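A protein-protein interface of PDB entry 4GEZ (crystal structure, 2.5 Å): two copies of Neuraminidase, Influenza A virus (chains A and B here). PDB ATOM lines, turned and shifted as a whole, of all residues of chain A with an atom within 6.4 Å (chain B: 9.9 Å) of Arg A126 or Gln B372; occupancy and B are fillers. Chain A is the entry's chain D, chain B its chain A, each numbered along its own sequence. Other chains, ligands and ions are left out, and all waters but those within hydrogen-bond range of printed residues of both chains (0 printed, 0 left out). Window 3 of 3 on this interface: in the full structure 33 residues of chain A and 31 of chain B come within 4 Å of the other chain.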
ATOM      1  N   ARG A 124      16.297  24.068  17.603  1.00  0.00           N
ATOM      2  CA  ARG A 124      15.116  23.231  17.514  1.00  0.00           C
ATOM      3  C   ARG A 124      15.454  22.246  16.410  1.00  0.00           C
ATOM      4  O   ARG A 124      16.493  22.380  15.762  1.00  0.00           O
ATOM      5  CB  ARG A 124      13.892  24.052  17.114  1.00  0.00           C
ATOM      6  CG  ARG A 124      13.525  25.198  18.047  1.00  0.00           C
ATOM      7  CD  ARG A 124      13.329  26.484  17.259  1.00  0.00           C
ATOM      8  NE  ARG A 124      13.444  27.678  18.092  1.00  0.00           N
ATOM      9  CZ  ARG A 124      12.417  28.240  18.722  1.00  0.00           C
ATOM     10  NH1 ARG A 124      11.201  27.725  18.595  1.00  0.00           N
ATOM     11  NH2 ARG A 124      12.597  29.324  19.464  1.00  0.00           N
ATOM     12  N   ASP A 125      14.587  21.264  16.187  1.00  0.00           N
ATOM     13  CA  ASP A 125      14.808  20.253  15.147  1.00  0.00           C
ATOM     14  C   ASP A 125      16.165  19.538  15.202  1.00  0.00           C
ATOM     15  O   ASP A 125      16.756  19.379  16.269  1.00  0.00           O
ATOM     16  CB  ASP A 125      14.541  20.808  13.735  1.00  0.00           C
ATOM     17  CG  ASP A 125      14.012  22.230  13.740  1.00  0.00           C
ATOM     18  OD1 ASP A 125      13.053  22.506  14.494  1.00  0.00           O
ATOM     19  OD2 ASP A 125      14.552  23.069  12.987  1.00  0.00           O
ATOM     20  N   ARG A 126      16.640  19.107  14.037  1.00  0.00           N
ATOM     21  CA  ARG A 126      17.773  18.188  13.935  1.00  0.00           C
ATOM     22  C   ARG A 126      19.138  18.832  14.210  1.00  0.00           C
ATOM     23  O   ARG A 126      20.086  18.154  14.614  1.00  0.00           O
ATOM     24  CB  ARG A 126      17.743  17.533  12.549  1.00  0.00           C
ATOM     25  CG  ARG A 126      16.336  17.540  11.946  1.00  0.00           C
ATOM     26  CD  ARG A 126      16.303  17.159  10.473  1.00  0.00           C
ATOM     27  NE  ARG A 126      17.186  16.041  10.161  1.00  0.00           N
ATOM     28  CZ  ARG A 126      17.759  15.842   8.978  1.00  0.00           C
ATOM     29  NH1 ARG A 126      17.560  16.698   7.984  1.00  0.00           N
ATOM     30  NH2 ARG A 126      18.544  14.790   8.796  1.00  0.00           N
ATOM     31  N   ASN A 127      19.221  20.145  14.023  1.00  0.00           N
ATOM     32  CA  ASN A 127      20.450  20.889  14.289  1.00  0.00           C
ATOM     33  C   ASN A 127      20.718  21.072  15.786  1.00  0.00           C
ATOM     34  O   ASN A 127      21.755  21.605  16.184  1.00  0.00           O
ATOM     35  CB  ASN A 127      20.422  22.236  13.564  1.00  0.00           C
ATOM     36  CG  ASN A 127      20.711  22.098  12.081  1.00  0.00           C
ATOM     37  OD1 ASN A 127      21.040  21.013  11.598  1.00  0.00           O
ATOM     38  ND2 ASN A 127      20.581  23.198  11.348  1.00  0.00           N
ATOM     39  N   SER A 128      19.764  20.648  16.607  1.00  0.00           N
ATOM     40  CA  SER A 128      19.903  20.714  18.057  1.00  0.00           C
ATOM     41  C   SER A 128      21.131  19.944  18.547  1.00  0.00           C
ATOM     42  O   SER A 128      21.461  18.877  18.018  1.00  0.00           O
ATOM     43  CB  SER A 128      18.646  20.169  18.740  1.00  0.00           C
ATOM     44  OG  SER A 128      18.780  20.204  20.147  1.00  0.00           O
ATOM     45  N   PHE A 129      21.816  20.501  19.543  1.00  0.00           N
ATOM     46  CA  PHE A 129      22.936  19.808  20.174  1.00  0.00           C
ATOM     47  C   PHE A 129      23.126  20.321  21.599  1.00  0.00           C
ATOM     48  O   PHE A 129      22.476  21.282  22.012  1.00  0.00           O
ATOM     49  CB  PHE A 129      24.224  19.989  19.372  1.00  0.00           C
ATOM     50  CG  PHE A 129      24.936  21.279  19.642  1.00  0.00           C
ATOM     51  CD1 PHE A 129      24.468  22.483  19.130  1.00  0.00           C
ATOM     52  CD2 PHE A 129      26.102  21.275  20.388  1.00  0.00           C
ATOM     53  CE1 PHE A 129      25.147  23.668  19.382  1.00  0.00           C
ATOM     54  CE2 PHE A 129      26.783  22.443  20.641  1.00  0.00           C
ATOM     55  CZ  PHE A 129      26.309  23.645  20.139  1.00  0.00           C
ATOM     56  N   SER A 143      25.263  15.966  19.409  1.00  0.00           N
ATOM     57  CA  SER A 143      24.141  16.476  18.630  1.00  0.00           C
ATOM     58  C   SER A 143      22.928  15.576  18.770  1.00  0.00           C
ATOM     59  O   SER A 143      23.028  14.461  19.277  1.00  0.00           O
ATOM     60  CB  SER A 143      24.525  16.604  17.151  1.00  0.00           C
ATOM     61  OG  SER A 143      25.634  17.467  16.978  1.00  0.00           O
ATOM     62  N   ALA A 144      21.786  16.055  18.297  1.00  0.00           N
ATOM     63  CA  ALA A 144      20.569  15.263  18.336  1.00  0.00           C
ATOM     64  C   ALA A 144      20.707  13.988  17.502  1.00  0.00           C
ATOM     65  O   ALA A 144      21.239  14.016  16.392  1.00  0.00           O
ATOM     66  CB  ALA A 144      19.411  16.090  17.841  1.00  0.00           C
ATOM     67  N   SER A 145      20.213  12.876  18.044  1.00  0.00           N
ATOM     68  CA  SER A 145      20.286  11.581  17.365  1.00  0.00           C
ATOM     69  C   SER A 145      18.917  11.152  16.841  1.00  0.00           C
ATOM     70  O   SER A 145      18.824  10.349  15.910  1.00  0.00           O
ATOM     71  CB  SER A 145      20.840  10.515  18.320  1.00  0.00           C
ATOM     72  OG  SER A 145      20.472   9.208  17.914  1.00  0.00           O
ATOM     73  N   GLY A 147      16.220  13.246  15.774  1.00  0.00           N
ATOM     74  CA  GLY A 147      15.460  14.214  15.000  1.00  0.00           C
ATOM     75  C   GLY A 147      14.945  15.440  15.733  1.00  0.00           C
ATOM     76  O   GLY A 147      15.245  16.566  15.339  1.00  0.00           O
ATOM     77  N   GLY A 148      14.187  15.225  16.807  1.00  0.00           N
ATOM     78  CA  GLY A 148      13.569  16.314  17.550  1.00  0.00           C
ATOM     79  C   GLY A 148      14.562  17.182  18.295  1.00  0.00           C
ATOM     80  O   GLY A 148      15.763  16.921  18.256  1.00  0.00           O
ATOM     81  N   PRO A 149      14.073  18.234  18.969  1.00  0.00           N
ATOM     82  CA  PRO A 149      15.009  19.094  19.700  1.00  0.00           C
ATOM     83  C   PRO A 149      15.545  18.389  20.941  1.00  0.00           C
ATOM     84  O   PRO A 149      14.789  17.681  21.607  1.00  0.00           O
ATOM     85  CB  PRO A 149      14.138  20.287  20.109  1.00  0.00           C
ATOM     86  CG  PRO A 149      12.749  19.738  20.168  1.00  0.00           C
ATOM     87  CD  PRO A 149      12.677  18.699  19.082  1.00  0.00           C
ATOM     88  N   LYS B  24      37.481  21.471  14.883  1.00  0.00           N
ATOM     89  CA  LYS B  24      36.514  20.936  13.927  1.00  0.00           C
ATOM     90  C   LYS B  24      35.239  21.761  13.921  1.00  0.00           C
ATOM     91  O   LYS B  24      34.378  21.599  13.051  1.00  0.00           O
ATOM     92  CB  LYS B  24      36.129  19.500  14.291  1.00  0.00           C
ATOM     93  CG  LYS B  24      37.224  18.457  14.255  1.00  0.00           C
ATOM     94  CD  LYS B  24      36.563  17.087  14.263  1.00  0.00           C
ATOM     95  CE  LYS B  24      37.527  15.942  14.033  1.00  0.00           C
ATOM     96  NZ  LYS B  24      36.759  14.673  13.866  1.00  0.00           N
ATOM     97  N   GLY B  25      35.119  22.647  14.901  1.00  0.00           N
ATOM     98  CA  GLY B  25      33.923  23.450  15.039  1.00  0.00           C
ATOM     99  C   GLY B  25      34.104  24.589  16.020  1.00  0.00           C
ATOM    100  O   GLY B  25      35.087  24.643  16.757  1.00  0.00           O
ATOM    101  N   TRP B  26      33.137  25.496  16.034  1.00  0.00           N
ATOM    102  CA  TRP B  26      33.186  26.654  16.908  1.00  0.00           C
ATOM    103  C   TRP B  26      31.861  26.724  17.653  1.00  0.00           C
ATOM    104  O   TRP B  26      30.793  26.658  17.037  1.00  0.00           O
ATOM    105  CB  TRP B  26      33.422  27.917  16.077  1.00  0.00           C
ATOM    106  CG  TRP B  26      34.627  27.810  15.179  1.00  0.00           C
ATOM    107  CD1 TRP B  26      34.664  27.301  13.909  1.00  0.00           C
ATOM    108  CD2 TRP B  26      35.963  28.221  15.485  1.00  0.00           C
ATOM    109  NE1 TRP B  26      35.944  27.368  13.411  1.00  0.00           N
ATOM    110  CE2 TRP B  26      36.762  27.931  14.359  1.00  0.00           C
ATOM    111  CE3 TRP B  26      36.567  28.807  16.603  1.00  0.00           C
ATOM    112  CZ2 TRP B  26      38.131  28.208  14.320  1.00  0.00           C
ATOM    113  CZ3 TRP B  26      37.921  29.081  16.564  1.00  0.00           C
ATOM    114  CH2 TRP B  26      38.689  28.782  15.432  1.00  0.00           C
ATOM    115  N   VAL B  27      31.930  26.835  18.977  1.00  0.00           N
ATOM    116  CA  VAL B  27      30.730  26.905  19.802  1.00  0.00           C
ATOM    117  C   VAL B  27      30.730  28.187  20.627  1.00  0.00           C
ATOM    118  O   VAL B  27      31.777  28.617  21.116  1.00  0.00           O
ATOM    119  CB  VAL B  27      30.585  25.663  20.729  1.00  0.00           C
ATOM    120  CG1 VAL B  27      30.213  24.432  19.920  1.00  0.00           C
ATOM    121  CG2 VAL B  27      31.864  25.419  21.506  1.00  0.00           C
ATOM    122  N   PRO B  28      29.551  28.802  20.782  1.00  0.00           N
ATOM    123  CA  PRO B  28      29.454  30.069  21.510  1.00  0.00           C
ATOM    124  C   PRO B  28      29.570  29.879  23.016  1.00  0.00           C
ATOM    125  O   PRO B  28      28.873  29.050  23.600  1.00  0.00           O
ATOM    126  CB  PRO B  28      28.054  30.572  21.140  1.00  0.00           C
ATOM    127  CG  PRO B  28      27.280  29.337  20.854  1.00  0.00           C
ATOM    128  CD  PRO B  28      28.255  28.380  20.222  1.00  0.00           C
ATOM    129  N   LEU B 313      35.197  22.296   5.196  1.00  0.00           N
ATOM    130  CA  LEU B 313      34.112  22.592   6.129  1.00  0.00           C
ATOM    131  C   LEU B 313      33.692  24.061   6.059  1.00  0.00           C
ATOM    132  O   LEU B 313      34.535  24.953   5.962  1.00  0.00           O
ATOM    133  CB  LEU B 313      34.543  22.244   7.558  1.00  0.00           C
ATOM    134  CG  LEU B 313      34.079  20.905   8.140  1.00  0.00           C
ATOM    135  CD1 LEU B 313      34.437  19.746   7.230  1.00  0.00           C
ATOM    136  CD2 LEU B 313      34.672  20.683   9.527  1.00  0.00           C
ATOM    137  N   SER B 314      32.383  24.303   6.097  1.00  0.00           N
ATOM    138  CA  SER B 314      31.838  25.663   6.055  1.00  0.00           C
ATOM    139  C   SER B 314      30.687  25.832   7.046  1.00  0.00           C
ATOM    140  O   SER B 314      29.618  25.249   6.865  1.00  0.00           O
ATOM    141  CB  SER B 314      31.351  25.991   4.637  1.00  0.00           C
ATOM    142  OG  SER B 314      30.973  27.351   4.515  1.00  0.00           O
ATOM    143  N   TYR B 315      30.895  26.633   8.088  1.00  0.00           N
ATOM    144  CA  TYR B 315      29.841  26.876   9.071  1.00  0.00           C
ATOM    145  C   TYR B 315      29.298  28.289   8.958  1.00  0.00           C
ATOM    146  O   TYR B 315      30.048  29.261   9.011  1.00  0.00           O
ATOM    147  CB  TYR B 315      30.355  26.639  10.494  1.00  0.00           C
ATOM    148  CG  TYR B 315      30.603  25.186  10.832  1.00  0.00           C
ATOM    149  CD1 TYR B 315      29.543  24.304  10.989  1.00  0.00           C
ATOM    150  CD2 TYR B 315      31.895  24.701  11.003  1.00  0.00           C
ATOM    151  CE1 TYR B 315      29.761  22.977  11.302  1.00  0.00           C
ATOM    152  CE2 TYR B 315      32.124  23.377  11.318  1.00  0.00           C
ATOM    153  CZ  TYR B 315      31.052  22.519  11.466  1.00  0.00           C
ATOM    154  OH  TYR B 315      31.270  21.198  11.780  1.00  0.00           O
ATOM    155  N   GLU B 316      27.987  28.394   8.799  1.00  0.00           N
ATOM    156  CA  GLU B 316      27.328  29.686   8.777  1.00  0.00           C
ATOM    157  C   GLU B 316      26.754  29.964  10.161  1.00  0.00           C
ATOM    158  O   GLU B 316      25.636  29.554  10.466  1.00  0.00           O
ATOM    159  CB  GLU B 316      26.225  29.693   7.721  1.00  0.00           C
ATOM    160  CG  GLU B 316      25.538  31.034   7.537  1.00  0.00           C
ATOM    161  CD  GLU B 316      24.601  31.043   6.348  1.00  0.00           C
ATOM    162  OE1 GLU B 316      23.405  31.349   6.537  1.00  0.00           O
ATOM    163  OE2 GLU B 316      25.064  30.750   5.226  1.00  0.00           O
ATOM    164  N   LEU B 317      27.533  30.649  10.998  1.00  0.00           N
ATOM    165  CA  LEU B 317      27.131  30.932  12.375  1.00  0.00           C
ATOM    166  C   LEU B 317      25.994  31.941  12.428  1.00  0.00           C
ATOM    167  O   LEU B 317      25.103  31.845  13.271  1.00  0.00           O
ATOM    168  CB  LEU B 317      28.319  31.459  13.193  1.00  0.00           C
ATOM    169  CG  LEU B 317      29.533  30.566  13.455  1.00  0.00           C
ATOM    170  CD1 LEU B 317      30.585  31.300  14.261  1.00  0.00           C
ATOM    171  CD2 LEU B 317      29.105  29.318  14.188  1.00  0.00           C
ATOM    172  N   PHE B 364      33.285  32.751  20.725  1.00  0.00           N
ATOM    173  CA  PHE B 364      33.207  31.372  20.259  1.00  0.00           C
ATOM    174  C   PHE B 364      34.544  30.682  20.538  1.00  0.00           C
ATOM    175  O   PHE B 364      35.600  31.313  20.460  1.00  0.00           O
ATOM    176  CB  PHE B 364      32.899  31.320  18.759  1.00  0.00           C
ATOM    177  CG  PHE B 364      31.484  31.703  18.404  1.00  0.00           C
ATOM    178  CD1 PHE B 364      31.105  33.040  18.331  1.00  0.00           C
ATOM    179  CD2 PHE B 364      30.536  30.723  18.122  1.00  0.00           C
ATOM    180  CE1 PHE B 364      29.804  33.396  17.990  1.00  0.00           C
ATOM    181  CE2 PHE B 364      29.232  31.068  17.782  1.00  0.00           C
ATOM    182  CZ  PHE B 364      28.866  32.409  17.717  1.00  0.00           C
ATOM    183  N   ILE B 367      36.411  23.555  18.918  1.00  0.00           N
ATOM    184  CA  ILE B 367      36.343  22.228  19.528  1.00  0.00           C
ATOM    185  C   ILE B 367      36.791  21.103  18.588  1.00  0.00           C
ATOM    186  O   ILE B 367      36.697  21.222  17.362  1.00  0.00           O
ATOM    187  CB  ILE B 367      34.916  21.912  20.032  1.00  0.00           C
ATOM    188  CG1 ILE B 367      33.876  22.185  18.942  1.00  0.00           C
ATOM    189  CG2 ILE B 367      34.609  22.699  21.296  1.00  0.00           C
ATOM    190  CD1 ILE B 367      32.489  21.654  19.274  1.00  0.00           C
ATOM    191  N   SER B 369      35.385  18.204  18.437  1.00  0.00           N
ATOM    192  CA  SER B 369      34.240  17.426  17.988  1.00  0.00           C
ATOM    193  C   SER B 369      33.544  18.201  16.883  1.00  0.00           C
ATOM    194  O   SER B 369      33.455  19.426  16.944  1.00  0.00           O
ATOM    195  CB  SER B 369      33.271  17.162  19.143  1.00  0.00           C
ATOM    196  OG  SER B 369      32.143  16.421  18.706  1.00  0.00           O
ATOM    197  N   PRO B 370      33.036  17.491  15.867  1.00  0.00           N
ATOM    198  CA  PRO B 370      32.223  18.200  14.878  1.00  0.00           C
ATOM    199  C   PRO B 370      30.906  18.588  15.524  1.00  0.00           C
ATOM    200  O   PRO B 370      30.469  17.920  16.461  1.00  0.00           O
ATOM    201  CB  PRO B 370      32.001  17.151  13.777  1.00  0.00           C
ATOM    202  CG  PRO B 370      33.046  16.100  14.011  1.00  0.00           C
ATOM    203  CD  PRO B 370      33.294  16.093  15.485  1.00  0.00           C
ATOM    204  N   VAL B 371      30.283  19.651  15.030  1.00  0.00           N
ATOM    205  CA  VAL B 371      29.076  20.181  15.649  1.00  0.00           C
ATOM    206  C   VAL B 371      28.076  20.501  14.542  1.00  0.00           C
ATOM    207  O   VAL B 371      28.458  20.636  13.381  1.00  0.00           O
ATOM    208  CB  VAL B 371      29.401  21.432  16.520  1.00  0.00           C
ATOM    209  CG1 VAL B 371      29.885  22.587  15.655  1.00  0.00           C
ATOM    210  CG2 VAL B 371      28.203  21.850  17.364  1.00  0.00           C
ATOM    211  N   GLN B 372      26.800  20.597  14.897  1.00  0.00           N
ATOM    212  CA  GLN B 372      25.758  20.913  13.930  1.00  0.00           C
ATOM    213  C   GLN B 372      25.997  22.276  13.297  1.00  0.00           C
ATOM    214  O   GLN B 372      26.520  23.179  13.947  1.00  0.00           O
ATOM    215  CB  GLN B 372      24.390  20.904  14.617  1.00  0.00           C
ATOM    216  CG  GLN B 372      23.970  19.545  15.137  1.00  0.00           C
ATOM    217  CD  GLN B 372      23.653  18.574  14.022  1.00  0.00           C
ATOM    218  OE1 GLN B 372      22.683  18.755  13.286  1.00  0.00           O
ATOM    219  NE2 GLN B 372      24.483  17.545  13.878  1.00  0.00           N
ATOM    220  N   ASN B 373      25.613  22.430  12.033  1.00  0.00           N
ATOM    221  CA  ASN B 373      25.703  23.734  11.385  1.00  0.00           C
ATOM    222  C   ASN B 373      24.491  24.569  11.773  1.00  0.00           C
ATOM    223  O   ASN B 373      23.651  24.891  10.933  1.00  0.00           O
ATOM    224  CB  ASN B 373      25.803  23.599   9.863  1.00  0.00           C
ATOM    225  CG  ASN B 373      26.186  24.907   9.181  1.00  0.00           C
ATOM    226  OD1 ASN B 373      26.646  25.844   9.829  1.00  0.00           O
ATOM    227  ND2 ASN B 373      25.993  24.973   7.870  1.00  0.00           N
ATOM    228  N   ILE B 374      24.425  24.926  13.054  1.00  0.00           N
ATOM    229  CA  ILE B 374      23.297  25.665  13.615  1.00  0.00           C
ATOM    230  C   ILE B 374      23.469  27.177  13.434  1.00  0.00           C
ATOM    231  O   ILE B 374      24.582  27.698  13.513  1.00  0.00           O
ATOM    232  CB  ILE B 374      23.102  25.289  15.114  1.00  0.00           C
ATOM    233  CG1 ILE B 374      22.071  26.195  15.785  1.00  0.00           C
ATOM    234  CG2 ILE B 374      24.427  25.338  15.858  1.00  0.00           C
ATOM    235  CD1 ILE B 374      21.937  25.992  17.284  1.00  0.00           C
ATOM    236  N   ASN B 375      22.361  27.869  13.168  1.00  0.00           N
ATOM    237  CA  ASN B 375      22.353  29.322  13.013  1.00  0.00           C
ATOM    238  C   ASN B 375      22.052  29.970  14.364  1.00  0.00           C
ATOM    239  O   ASN B 375      21.070  29.618  15.018  1.00  0.00           O
ATOM    240  CB  ASN B 375      21.290  29.727  11.983  1.00  0.00           C
ATOM    241  CG  ASN B 375      21.283  31.224  11.684  1.00  0.00           C
ATOM    242  OD1 ASN B 375      21.716  32.042  12.493  1.00  0.00           O
ATOM    243  ND2 ASN B 375      20.768  31.584  10.516  1.00  0.00           N
ATOM    244  N   TRP B 376      22.899  30.906  14.786  1.00  0.00           N
ATOM    245  CA  TRP B 376      22.739  31.562  16.084  1.00  0.00           C
ATOM    246  C   TRP B 376      21.941  32.871  16.052  1.00  0.00           C
ATOM    247  O   TRP B 376      22.001  33.660  16.997  1.00  0.00           O
ATOM    248  CB  TRP B 376      24.108  31.758  16.746  1.00  0.00           C
ATOM    249  CG  TRP B 376      24.742  30.447  17.098  1.00  0.00           C
ATOM    250  CD1 TRP B 376      25.735  29.795  16.421  1.00  0.00           C
ATOM    251  CD2 TRP B 376      24.396  29.612  18.205  1.00  0.00           C
ATOM    252  NE1 TRP B 376      26.033  28.609  17.050  1.00  0.00           N
ATOM    253  CE2 TRP B 376      25.222  28.472  18.148  1.00  0.00           C
ATOM    254  CE3 TRP B 376      23.469  29.719  19.244  1.00  0.00           C
ATOM    255  CZ2 TRP B 376      25.144  27.445  19.092  1.00  0.00           C
ATOM    256  CZ3 TRP B 376      23.398  28.709  20.179  1.00  0.00           C
ATOM    257  CH2 TRP B 376      24.231  27.590  20.102  1.00  0.00           C
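The backbone carbonyl oxygen of Gly A147 is in hydrogen-bond range of the backbone NH of Arg A126, 3.2 Å away.
OD1 of Asn B373 is in hydrogen-bond range of N of Glu B316 (3.1 Å).
The backbone carbonyl oxygen (O) of Ser A128 sits at hydrogen-bond distance from the backbone NH (N) of Ala A144 (2.9 Å).
OH of Tyr B315 sits at hydrogen-bond distance from O of Val B371 (3.3 Å).
The backbone carbonyl oxygen (O) of Leu B317 lies within hydrogen-bond range of the backbone NH (N) of Trp B376 (2.8 Å).
No position is printed for both chains.
Of the 9 pairs that touch across the chains among the printed residues, none has its exchanged pair printed and touching as well.
No residue of chain B comes within 4 Å of Asp A125.
Arg A126 touches one residue of chain B.
No residue of chain B comes within 4 Å of Ala A144.
No residue of chain B comes within 4 Å of Gly A147.
No residue of chain B comes within 4 Å of Gly A148.
Glu B316 touches none of the printed residues of chain A.
Of the printed residues of chain A, Val B371 touches Phe A129 (3.6 Å).
Gln B372 touches four residues of chain A.
Printed residues of chain A within 4 Å of Ile B374: Phe A129.
The nearest residue of chain B that does not touch Arg A126 is Asn B373 (7.4 Å).
The nearest printed residue of chain B that does not touch Phe A129 is Gln B372 (4.3 Å).
Of the 20 printed residues of chain B, 6 touch a printed residue of chain A.
Printed residues of chain B that touch a printed residue of chain A: Val B27, Val B371, Gln B372, Asn B373, Ile B374 and Trp B376.
Among the printed residues, no Asp or Glu carboxylate lies within 4 Å of a Lys or Arg side-chain nitrogen of the other chain.
Among the printed residues, merely in contact across the chains: Asn A127 with Asn B373, Ser A128 with Gln B372, Phe A129 with Val B27, Phe A129 with Val B371, Phe A129 with Ile B374 and Phe A129 with Trp B376.
The side-chain amide nitrogen of Gln B372 sits close to the side-chain hydroxyl of Ser A143, at 3.3 Å.
The side-chain amide oxygen (OE1) of Gln B372 lies close to the backbone carbonyl oxygen (O) of Arg A126.
OD1 of Asn A127 lies close to OE1 of Gln B372 (3.3 Å).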
